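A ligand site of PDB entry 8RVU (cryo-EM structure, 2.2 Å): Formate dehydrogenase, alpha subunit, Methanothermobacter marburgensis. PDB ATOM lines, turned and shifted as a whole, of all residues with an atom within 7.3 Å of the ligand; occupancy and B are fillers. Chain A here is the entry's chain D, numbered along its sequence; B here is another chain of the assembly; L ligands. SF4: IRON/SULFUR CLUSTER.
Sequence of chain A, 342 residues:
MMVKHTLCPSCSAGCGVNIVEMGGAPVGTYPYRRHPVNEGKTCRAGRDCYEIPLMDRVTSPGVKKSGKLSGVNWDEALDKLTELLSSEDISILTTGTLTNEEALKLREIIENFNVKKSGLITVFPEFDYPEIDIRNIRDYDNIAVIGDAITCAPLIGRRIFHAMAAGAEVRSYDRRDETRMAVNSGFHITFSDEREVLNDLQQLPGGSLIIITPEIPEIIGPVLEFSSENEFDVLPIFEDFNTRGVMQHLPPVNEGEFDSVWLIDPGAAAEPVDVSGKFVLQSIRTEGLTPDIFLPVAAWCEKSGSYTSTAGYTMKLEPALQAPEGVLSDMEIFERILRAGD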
ATOM      1  N   LEU A   7      36.422 -28.724 -13.712  1.00  0.00           N
ATOM      2  CA  LEU A   7      35.183 -29.435 -13.990  1.00  0.00           C
ATOM      3  C   LEU A   7      34.284 -29.422 -12.759  1.00  0.00           C
ATOM      4  O   LEU A   7      34.753 -29.453 -11.620  1.00  0.00           O
ATOM      5  CB  LEU A   7      35.491 -30.876 -14.397  1.00  0.00           C
ATOM      6  CG  LEU A   7      34.341 -31.879 -14.482  1.00  0.00           C
ATOM      7  CD1 LEU A   7      33.561 -31.716 -15.781  1.00  0.00           C
ATOM      8  CD2 LEU A   7      34.853 -33.307 -14.331  1.00  0.00           C
ATOM      9  N   CYS A   8      32.976 -29.367 -13.004  1.00  0.00           N
ATOM     10  CA  CYS A   8      32.009 -29.476 -11.929  1.00  0.00           C
ATOM     11  C   CYS A   8      31.838 -30.938 -11.533  1.00  0.00           C
ATOM     12  O   CYS A   8      31.520 -31.765 -12.402  1.00  0.00           O
ATOM     13  CB  CYS A   8      30.670 -28.885 -12.336  1.00  0.00           C
ATOM     14  SG  CYS A   8      29.351 -29.205 -11.154  1.00  0.00           S
ATOM     15  N   PRO A   9      32.037 -31.309 -10.269  1.00  0.00           N
ATOM     16  CA  PRO A   9      31.935 -32.720  -9.879  1.00  0.00           C
ATOM     17  C   PRO A   9      30.565 -33.163  -9.398  1.00  0.00           C
ATOM     18  O   PRO A   9      30.427 -34.322  -9.006  1.00  0.00           O
ATOM     19  CB  PRO A   9      32.948 -32.794  -8.733  1.00  0.00           C
ATOM     20  CG  PRO A   9      32.804 -31.469  -8.060  1.00  0.00           C
ATOM     21  CD  PRO A   9      32.433 -30.470  -9.131  1.00  0.00           C
ATOM     22  N   SER A  10      29.562 -32.295  -9.433  1.00  0.00           N
ATOM     23  CA  SER A  10      28.312 -32.572  -8.728  1.00  0.00           C
ATOM     24  C   SER A  10      27.441 -33.593  -9.457  1.00  0.00           C
ATOM     25  O   SER A  10      26.717 -34.341  -8.793  1.00  0.00           O
ATOM     26  CB  SER A  10      27.534 -31.267  -8.517  1.00  0.00           C
ATOM     27  OG  SER A  10      28.251 -30.418  -7.635  1.00  0.00           O
ATOM     28  N   CYS A  11      27.492 -33.639 -10.784  1.00  0.00           N
ATOM     29  CA  CYS A  11      26.792 -34.677 -11.541  1.00  0.00           C
ATOM     30  C   CYS A  11      27.630 -35.037 -12.759  1.00  0.00           C
ATOM     31  O   CYS A  11      28.759 -34.568 -12.921  1.00  0.00           O
ATOM     32  CB  CYS A  11      25.382 -34.233 -11.947  1.00  0.00           C
ATOM     33  SG  CYS A  11      25.288 -33.302 -13.491  1.00  0.00           S
ATOM     34  N   SER A  12      27.066 -35.883 -13.610  1.00  0.00           N
ATOM     35  CA  SER A  12      27.818 -36.454 -14.724  1.00  0.00           C
ATOM     36  C   SER A  12      27.856 -35.560 -15.958  1.00  0.00           C
ATOM     37  O   SER A  12      28.567 -35.904 -16.912  1.00  0.00           O
ATOM     38  CB  SER A  12      27.245 -37.821 -15.089  1.00  0.00           C
ATOM     39  OG  SER A  12      25.837 -37.767 -15.232  1.00  0.00           O
ATOM     40  N   ALA A  13      27.129 -34.452 -15.973  1.00  0.00           N
ATOM     41  CA  ALA A  13      27.311 -33.488 -17.044  1.00  0.00           C
ATOM     42  C   ALA A  13      28.702 -32.878 -16.957  1.00  0.00           C
ATOM     43  O   ALA A  13      29.213 -32.612 -15.875  1.00  0.00           O
ATOM     44  CB  ALA A  13      26.241 -32.398 -16.962  1.00  0.00           C
ATOM     45  N   GLY A  14      29.326 -32.670 -18.113  1.00  0.00           N
ATOM     46  CA  GLY A  14      30.693 -32.194 -18.140  1.00  0.00           C
ATOM     47  C   GLY A  14      30.825 -30.683 -18.096  1.00  0.00           C
ATOM     48  O   GLY A  14      31.658 -30.111 -18.792  1.00  0.00           O
ATOM     49  N   CYS A  15      30.014 -30.031 -17.271  1.00  0.00           N
ATOM     50  CA  CYS A  15      30.015 -28.569 -17.225  1.00  0.00           C
ATOM     51  C   CYS A  15      31.334 -28.055 -16.659  1.00  0.00           C
ATOM     52  O   CYS A  15      31.866 -28.579 -15.689  1.00  0.00           O
ATOM     53  CB  CYS A  15      28.854 -28.072 -16.369  1.00  0.00           C
ATOM     54  SG  CYS A  15      27.228 -28.525 -17.001  1.00  0.00           S
ATOM     55  N   GLY A  16      31.857 -27.000 -17.291  1.00  0.00           N
ATOM     56  CA  GLY A  16      33.070 -26.355 -16.820  1.00  0.00           C
ATOM     57  C   GLY A  16      32.754 -25.149 -15.951  1.00  0.00           C
ATOM     58  O   GLY A  16      31.778 -24.432 -16.185  1.00  0.00           O
ATOM     59  N   VAL A  17      33.598 -24.931 -14.943  1.00  0.00           N
ATOM     60  CA  VAL A  17      33.477 -23.806 -14.032  1.00  0.00           C
ATOM     61  C   VAL A  17      34.862 -23.202 -13.829  1.00  0.00           C
ATOM     62  O   VAL A  17      35.864 -23.779 -14.241  1.00  0.00           O
ATOM     63  CB  VAL A  17      32.868 -24.217 -12.667  1.00  0.00           C
ATOM     64  CG1 VAL A  17      31.505 -24.851 -12.866  1.00  0.00           C
ATOM     65  CG2 VAL A  17      33.798 -25.175 -11.924  1.00  0.00           C
ATOM     66  N   VAL A  37      30.295 -27.630 -23.217  1.00  0.00           N
ATOM     67  CA  VAL A  37      29.160 -28.366 -22.674  1.00  0.00           C
ATOM     68  C   VAL A  37      28.086 -27.418 -22.184  1.00  0.00           C
ATOM     69  O   VAL A  37      26.893 -27.634 -22.424  1.00  0.00           O
ATOM     70  CB  VAL A  37      29.641 -29.316 -21.557  1.00  0.00           C
ATOM     71  CG1 VAL A  37      28.470 -29.729 -20.666  1.00  0.00           C
ATOM     72  CG2 VAL A  37      30.310 -30.537 -22.151  1.00  0.00           C
ATOM     73  N   ASN A  38      28.471 -26.350 -21.484  1.00  0.00           N
ATOM     74  CA  ASN A  38      27.519 -25.452 -20.847  1.00  0.00           C
ATOM     75  C   ASN A  38      27.718 -23.981 -21.164  1.00  0.00           C
ATOM     76  O   ASN A  38      26.829 -23.182 -20.851  1.00  0.00           O
ATOM     77  CB  ASN A  38      27.557 -25.634 -19.320  1.00  0.00           C
ATOM     78  CG  ASN A  38      28.920 -25.346 -18.730  1.00  0.00           C
ATOM     79  OD1 ASN A  38      29.949 -25.723 -19.299  1.00  0.00           O
ATOM     80  ND2 ASN A  38      28.946 -24.683 -17.585  1.00  0.00           N
ATOM     81  N   LYS A  41      27.183 -21.642 -18.243  1.00  0.00           N
ATOM     82  CA  LYS A  41      25.931 -21.760 -17.517  1.00  0.00           C
ATOM     83  C   LYS A  41      26.015 -22.945 -16.563  1.00  0.00           C
ATOM     84  O   LYS A  41      26.448 -24.026 -16.953  1.00  0.00           O
ATOM     85  CB  LYS A  41      24.745 -21.933 -18.481  1.00  0.00           C
ATOM     86  CG  LYS A  41      24.642 -20.853 -19.536  1.00  0.00           C
ATOM     87  CD  LYS A  41      23.744 -21.298 -20.682  1.00  0.00           C
ATOM     88  CE  LYS A  41      23.575 -20.196 -21.723  1.00  0.00           C
ATOM     89  NZ  LYS A  41      22.699 -19.098 -21.221  1.00  0.00           N
ATOM     90  N   THR A  42      25.600 -22.728 -15.313  1.00  0.00           N
ATOM     91  CA  THR A  42      25.652 -23.769 -14.308  1.00  0.00           C
ATOM     92  C   THR A  42      24.388 -23.749 -13.469  1.00  0.00           C
ATOM     93  O   THR A  42      23.735 -22.708 -13.320  1.00  0.00           O
ATOM     94  CB  THR A  42      26.867 -23.603 -13.372  1.00  0.00           C
ATOM     95  OG1 THR A  42      26.983 -22.231 -12.976  1.00  0.00           O
ATOM     96  CG2 THR A  42      28.140 -24.027 -14.075  1.00  0.00           C
ATOM     97  N   CYS A  43      24.035 -24.918 -12.930  1.00  0.00           N
ATOM     98  CA  CYS A  43      23.006 -24.994 -11.913  1.00  0.00           C
ATOM     99  C   CYS A  43      23.597 -24.599 -10.558  1.00  0.00           C
ATOM    100  O   CYS A  43      24.756 -24.183 -10.466  1.00  0.00           O
ATOM    101  CB  CYS A  43      22.411 -26.400 -11.867  1.00  0.00           C
ATOM    102  SG  CYS A  43      23.495 -27.643 -11.129  1.00  0.00           S
ATOM    103  N   ARG A  44      22.792 -24.710  -9.508  1.00  0.00           N
ATOM    104  CA  ARG A  44      23.246 -24.269  -8.189  1.00  0.00           C
ATOM    105  C   ARG A  44      24.460 -25.060  -7.728  1.00  0.00           C
ATOM    106  O   ARG A  44      25.403 -24.493  -7.154  1.00  0.00           O
ATOM    107  CB  ARG A  44      22.108 -24.389  -7.180  1.00  0.00           C
ATOM    108  CG  ARG A  44      22.285 -23.515  -5.951  1.00  0.00           C
ATOM    109  CD  ARG A  44      21.871 -22.090  -6.241  1.00  0.00           C
ATOM    110  NE  ARG A  44      22.108 -21.201  -5.106  1.00  0.00           N
ATOM    111  CZ  ARG A  44      21.306 -21.075  -4.062  1.00  0.00           C
ATOM    112  NH1 ARG A  44      20.183 -21.772  -3.973  1.00  0.00           N
ATOM    113  NH2 ARG A  44      21.627 -20.233  -3.096  1.00  0.00           N
ATOM    114  N   ALA A  45      24.462 -26.374  -7.953  1.00  0.00           N
ATOM    115  CA  ALA A  45      25.568 -27.209  -7.501  1.00  0.00           C
ATOM    116  C   ALA A  45      26.873 -26.807  -8.179  1.00  0.00           C
ATOM    117  O   ALA A  45      27.941 -26.837  -7.544  1.00  0.00           O
ATOM    118  CB  ALA A  45      25.251 -28.679  -7.759  1.00  0.00           C
ATOM    119  N   GLY A  46      26.822 -26.445  -9.453  1.00  0.00           N
ATOM    120  CA  GLY A  46      28.021 -26.011 -10.145  1.00  0.00           C
ATOM    121  C   GLY A  46      28.626 -24.764  -9.518  1.00  0.00           C
ATOM    122  O   GLY A  46      29.854 -24.617  -9.466  1.00  0.00           O
ATOM    123  N   ARG A  47      27.772 -23.853  -9.046  1.00  0.00           N
ATOM    124  CA  ARG A  47      28.263 -22.643  -8.396  1.00  0.00           C
ATOM    125  C   ARG A  47      28.610 -22.868  -6.923  1.00  0.00           C
ATOM    126  O   ARG A  47      29.289 -22.032  -6.332  1.00  0.00           O
ATOM    127  CB  ARG A  47      27.223 -21.530  -8.525  1.00  0.00           C
ATOM    128  CG  ARG A  47      27.469 -20.612  -9.718  1.00  0.00           C
ATOM    129  CD  ARG A  47      26.240 -19.808 -10.093  1.00  0.00           C
ATOM    130  NE  ARG A  47      25.196 -20.636 -10.688  1.00  0.00           N
ATOM    131  CZ  ARG A  47      24.006 -20.875 -10.152  1.00  0.00           C
ATOM    132  NH1 ARG A  47      23.658 -20.367  -8.979  1.00  0.00           N
ATOM    133  NH2 ARG A  47      23.138 -21.638 -10.816  1.00  0.00           N
ATOM    134  N   CYS A  49      30.169 -25.806  -5.964  1.00  0.00           N
ATOM    135  CA  CYS A  49      31.231 -26.809  -5.901  1.00  0.00           C
ATOM    136  C   CYS A  49      32.519 -26.272  -5.274  1.00  0.00           C
ATOM    137  O   CYS A  49      33.335 -27.065  -4.815  1.00  0.00           O
ATOM    138  CB  CYS A  49      31.529 -27.333  -7.311  1.00  0.00           C
ATOM    139  SG  CYS A  49      32.491 -26.223  -8.353  1.00  0.00           S
ATOM    140  N   ILE A 150      16.049 -33.554 -16.566  1.00  0.00           N
ATOM    141  CA  ILE A 150      16.370 -32.169 -16.262  1.00  0.00           C
ATOM    142  C   ILE A 150      16.940 -32.056 -14.849  1.00  0.00           C
ATOM    143  O   ILE A 150      17.958 -31.406 -14.619  1.00  0.00           O
ATOM    144  CB  ILE A 150      15.130 -31.274 -16.447  1.00  0.00           C
ATOM    145  CG1 ILE A 150      14.723 -31.212 -17.910  1.00  0.00           C
ATOM    146  CG2 ILE A 150      15.405 -29.876 -15.921  1.00  0.00           C
ATOM    147  CD1 ILE A 150      13.276 -30.839 -18.129  1.00  0.00           C
ATOM    148  N   THR A 151      16.268 -32.690 -13.882  1.00  0.00           N
ATOM    149  CA  THR A 151      16.755 -32.638 -12.508  1.00  0.00           C
ATOM    150  C   THR A 151      18.093 -33.358 -12.357  1.00  0.00           C
ATOM    151  O   THR A 151      18.995 -32.871 -11.670  1.00  0.00           O
ATOM    152  CB  THR A 151      15.716 -33.239 -11.561  1.00  0.00           C
ATOM    153  OG1 THR A 151      14.425 -32.675 -11.849  1.00  0.00           O
ATOM    154  CG2 THR A 151      16.080 -32.948 -10.109  1.00  0.00           C
ATOM    155  N   CYS A 152      18.238 -34.515 -13.007  1.00  0.00           N
ATOM    156  CA  CYS A 152      19.485 -35.270 -12.901  1.00  0.00           C
ATOM    157  C   CYS A 152      20.647 -34.493 -13.491  1.00  0.00           C
ATOM    158  O   CYS A 152      21.742 -34.448 -12.915  1.00  0.00           O
ATOM    159  CB  CYS A 152      19.323 -36.628 -13.596  1.00  0.00           C
ATOM    160  SG  CYS A 152      18.290 -37.806 -12.704  1.00  0.00           S
ATOM    161  N   ALA A 153      20.434 -33.854 -14.642  1.00  0.00           N
ATOM    162  CA  ALA A 153      21.472 -33.090 -15.326  1.00  0.00           C
ATOM    163  C   ALA A 153      20.833 -31.886 -15.991  1.00  0.00           C
ATOM    164  O   ALA A 153      20.396 -31.951 -17.149  1.00  0.00           O
ATOM    165  CB  ALA A 153      22.217 -33.945 -16.347  1.00  0.00           C
ATOM    166  N   PRO A 154      20.737 -30.758 -15.281  1.00  0.00           N
ATOM    167  CA  PRO A 154      20.055 -29.586 -15.851  1.00  0.00           C
ATOM    168  C   PRO A 154      20.612 -29.138 -17.194  1.00  0.00           C
ATOM    169  O   PRO A 154      19.840 -28.715 -18.063  1.00  0.00           O
ATOM    170  CB  PRO A 154      20.263 -28.512 -14.788  1.00  0.00           C
ATOM    171  CG  PRO A 154      20.310 -29.273 -13.508  1.00  0.00           C
ATOM    172  CD  PRO A 154      20.984 -30.584 -13.837  1.00  0.00           C
ATOM    173  N   LEU A 155      21.924 -29.227 -17.404  1.00  0.00           N
ATOM    174  CA  LEU A 155      22.508 -28.741 -18.646  1.00  0.00           C
ATOM    175  C   LEU A 155      22.357 -29.724 -19.800  1.00  0.00           C
ATOM    176  O   LEU A 155      22.661 -29.366 -20.943  1.00  0.00           O
ATOM    177  CB  LEU A 155      23.986 -28.412 -18.429  1.00  0.00           C
ATOM    178  CG  LEU A 155      24.302 -26.964 -18.038  1.00  0.00           C
ATOM    179  CD1 LEU A 155      23.837 -25.966 -19.088  1.00  0.00           C
ATOM    180  CD2 LEU A 155      23.678 -26.621 -16.686  1.00  0.00           C
ATOM    181  N   ILE A 156      21.883 -30.942 -19.533  1.00  0.00           N
ATOM    182  CA  ILE A 156      21.426 -31.825 -20.598  1.00  0.00           C
ATOM    183  C   ILE A 156      19.943 -31.612 -20.877  1.00  0.00           C
ATOM    184  O   ILE A 156      19.494 -31.717 -22.028  1.00  0.00           O
ATOM    185  CB  ILE A 156      21.722 -33.289 -20.263  1.00  0.00           C
ATOM    186  CG1 ILE A 156      23.226 -33.554 -20.365  1.00  0.00           C
ATOM    187  CG2 ILE A 156      20.965 -34.221 -21.201  1.00  0.00           C
ATOM    188  CD1 ILE A 156      23.677 -34.804 -19.653  1.00  0.00           C
ATOM    189  N   PHE A 241      30.723 -37.877 -11.876  1.00  0.00           N
ATOM    190  CA  PHE A 241      31.236 -37.057 -12.954  1.00  0.00           C
ATOM    191  C   PHE A 241      32.241 -37.772 -13.836  1.00  0.00           C
ATOM    192  O   PHE A 241      32.576 -37.253 -14.911  1.00  0.00           O
ATOM    193  CB  PHE A 241      31.854 -35.771 -12.393  1.00  0.00           C
ATOM    194  CG  PHE A 241      33.048 -35.985 -11.524  1.00  0.00           C
ATOM    195  CD1 PHE A 241      32.913 -36.268 -10.177  1.00  0.00           C
ATOM    196  CD2 PHE A 241      34.326 -35.901 -12.049  1.00  0.00           C
ATOM    197  CE1 PHE A 241      34.017 -36.459  -9.370  1.00  0.00           C
ATOM    198  CE2 PHE A 241      35.435 -36.093 -11.251  1.00  0.00           C
ATOM    199  CZ  PHE A 241      35.282 -36.377  -9.916  1.00  0.00           C
ATOM    200  N   ILE B 281      14.514 -23.362 -13.582  1.00  0.00           N
ATOM    201  CA  ILE B 281      14.862 -24.425 -12.654  1.00  0.00           C
ATOM    202  C   ILE B 281      15.241 -23.877 -11.285  1.00  0.00           C
ATOM    203  O   ILE B 281      15.713 -24.639 -10.433  1.00  0.00           O
ATOM    204  CB  ILE B 281      15.985 -25.312 -13.225  1.00  0.00           C
ATOM    205  CG1 ILE B 281      17.176 -24.452 -13.668  1.00  0.00           C
ATOM    206  CG2 ILE B 281      15.471 -26.148 -14.381  1.00  0.00           C
ATOM    207  CD1 ILE B 281      18.505 -25.140 -13.501  1.00  0.00           C
HETATM  208 FE1  SF4 L   1      26.527 -28.858 -14.859  1.00  0.00          FE
HETATM  209 FE2  SF4 L   1      24.761 -28.597 -12.782  1.00  0.00          FE
HETATM  210 FE3  SF4 L   1      27.369 -29.278 -12.288  1.00  0.00          FE
HETATM  211 FE4  SF4 L   1      25.684 -31.073 -13.486  1.00  0.00          FE
HETATM  212  S1  SF4 L   1      25.502 -30.234 -11.372  1.00  0.00           S
HETATM  213  S2  SF4 L   1      27.817 -30.579 -14.111  1.00  0.00           S
HETATM  214  S3  SF4 L   1      24.398 -29.679 -14.747  1.00  0.00           S
HETATM  215  S4  SF4 L   1      26.614 -27.323 -13.179  1.00  0.00           S
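An iron atom (FE4) of the ligand is bound by the side-chain sulfur of Cys 11, at 2.3 Å. An iron atom (FE2) of the ligand is bound by the side-chain sulfur (SG) of Cys 43 (2.3 Å). SG of Cys 15 is bound to FE1 of the ligand. S3 of the ligand lies close to N of Leu 155 (3.7 Å). An iron atom (FE3) of the ligand is bound by the side-chain sulfur (SG) of Cys 8, 2.3 Å away. The backbone NH (N) of Cys 43 lies close to a sulfur (S4) of the ligand (3.5 Å).
The backbone carbonyl oxygen (O) of Cys 43 lies close to the guanidinium group (NH2) of Arg 47 (3.0 Å). The backbone NH of Ala 13 sits close to the side-chain sulfur of Cys 11, 3.3 Å away. NH2 of Arg 47 lies within hydrogen-bond range of O of Thr 42, 2.8 Å away. SG of Cys 8 sits close to N of Ser 10. The backbone NH of Ala 45 sits close to the side-chain sulfur of Cys 43 (3.6 Å). O of Gly 46 is in hydrogen-bond range of SG of Cys 49 (3.3 Å). The backbone carbonyl oxygen (O) of Cys 152 sits close to the side-chain sulfur (SG) of Cys 11, 3.8 Å away. N of Cys 8 sits at hydrogen-bond distance from O of Cys 15 (3.0 Å).
S2 of the ligand sits close to O of Ala 13, 3.0 Å away. Merely in contact with the ligand: Ser 10 (3.7 Å), Thr 42 (3.7 Å), Ala 45 (3.9 Å), Gly 46 (3.6 Å) and Pro 154 (3.6 Å). Hydrophobic or aromatic side chains within 4 Å of the ligand: Ala 13, Ala 45, Pro 154 and Leu 155. 11 residues have an atom within 4 Å of the ligand: Cys 8, Ser 10, Cys 11, Ala 13, Cys 15, Thr 42, Cys 43, Ala 45, Gly 46, Pro 154 and Leu 155. Along chain A the residues within 4 Å of the ligand span positions 8 to 155.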
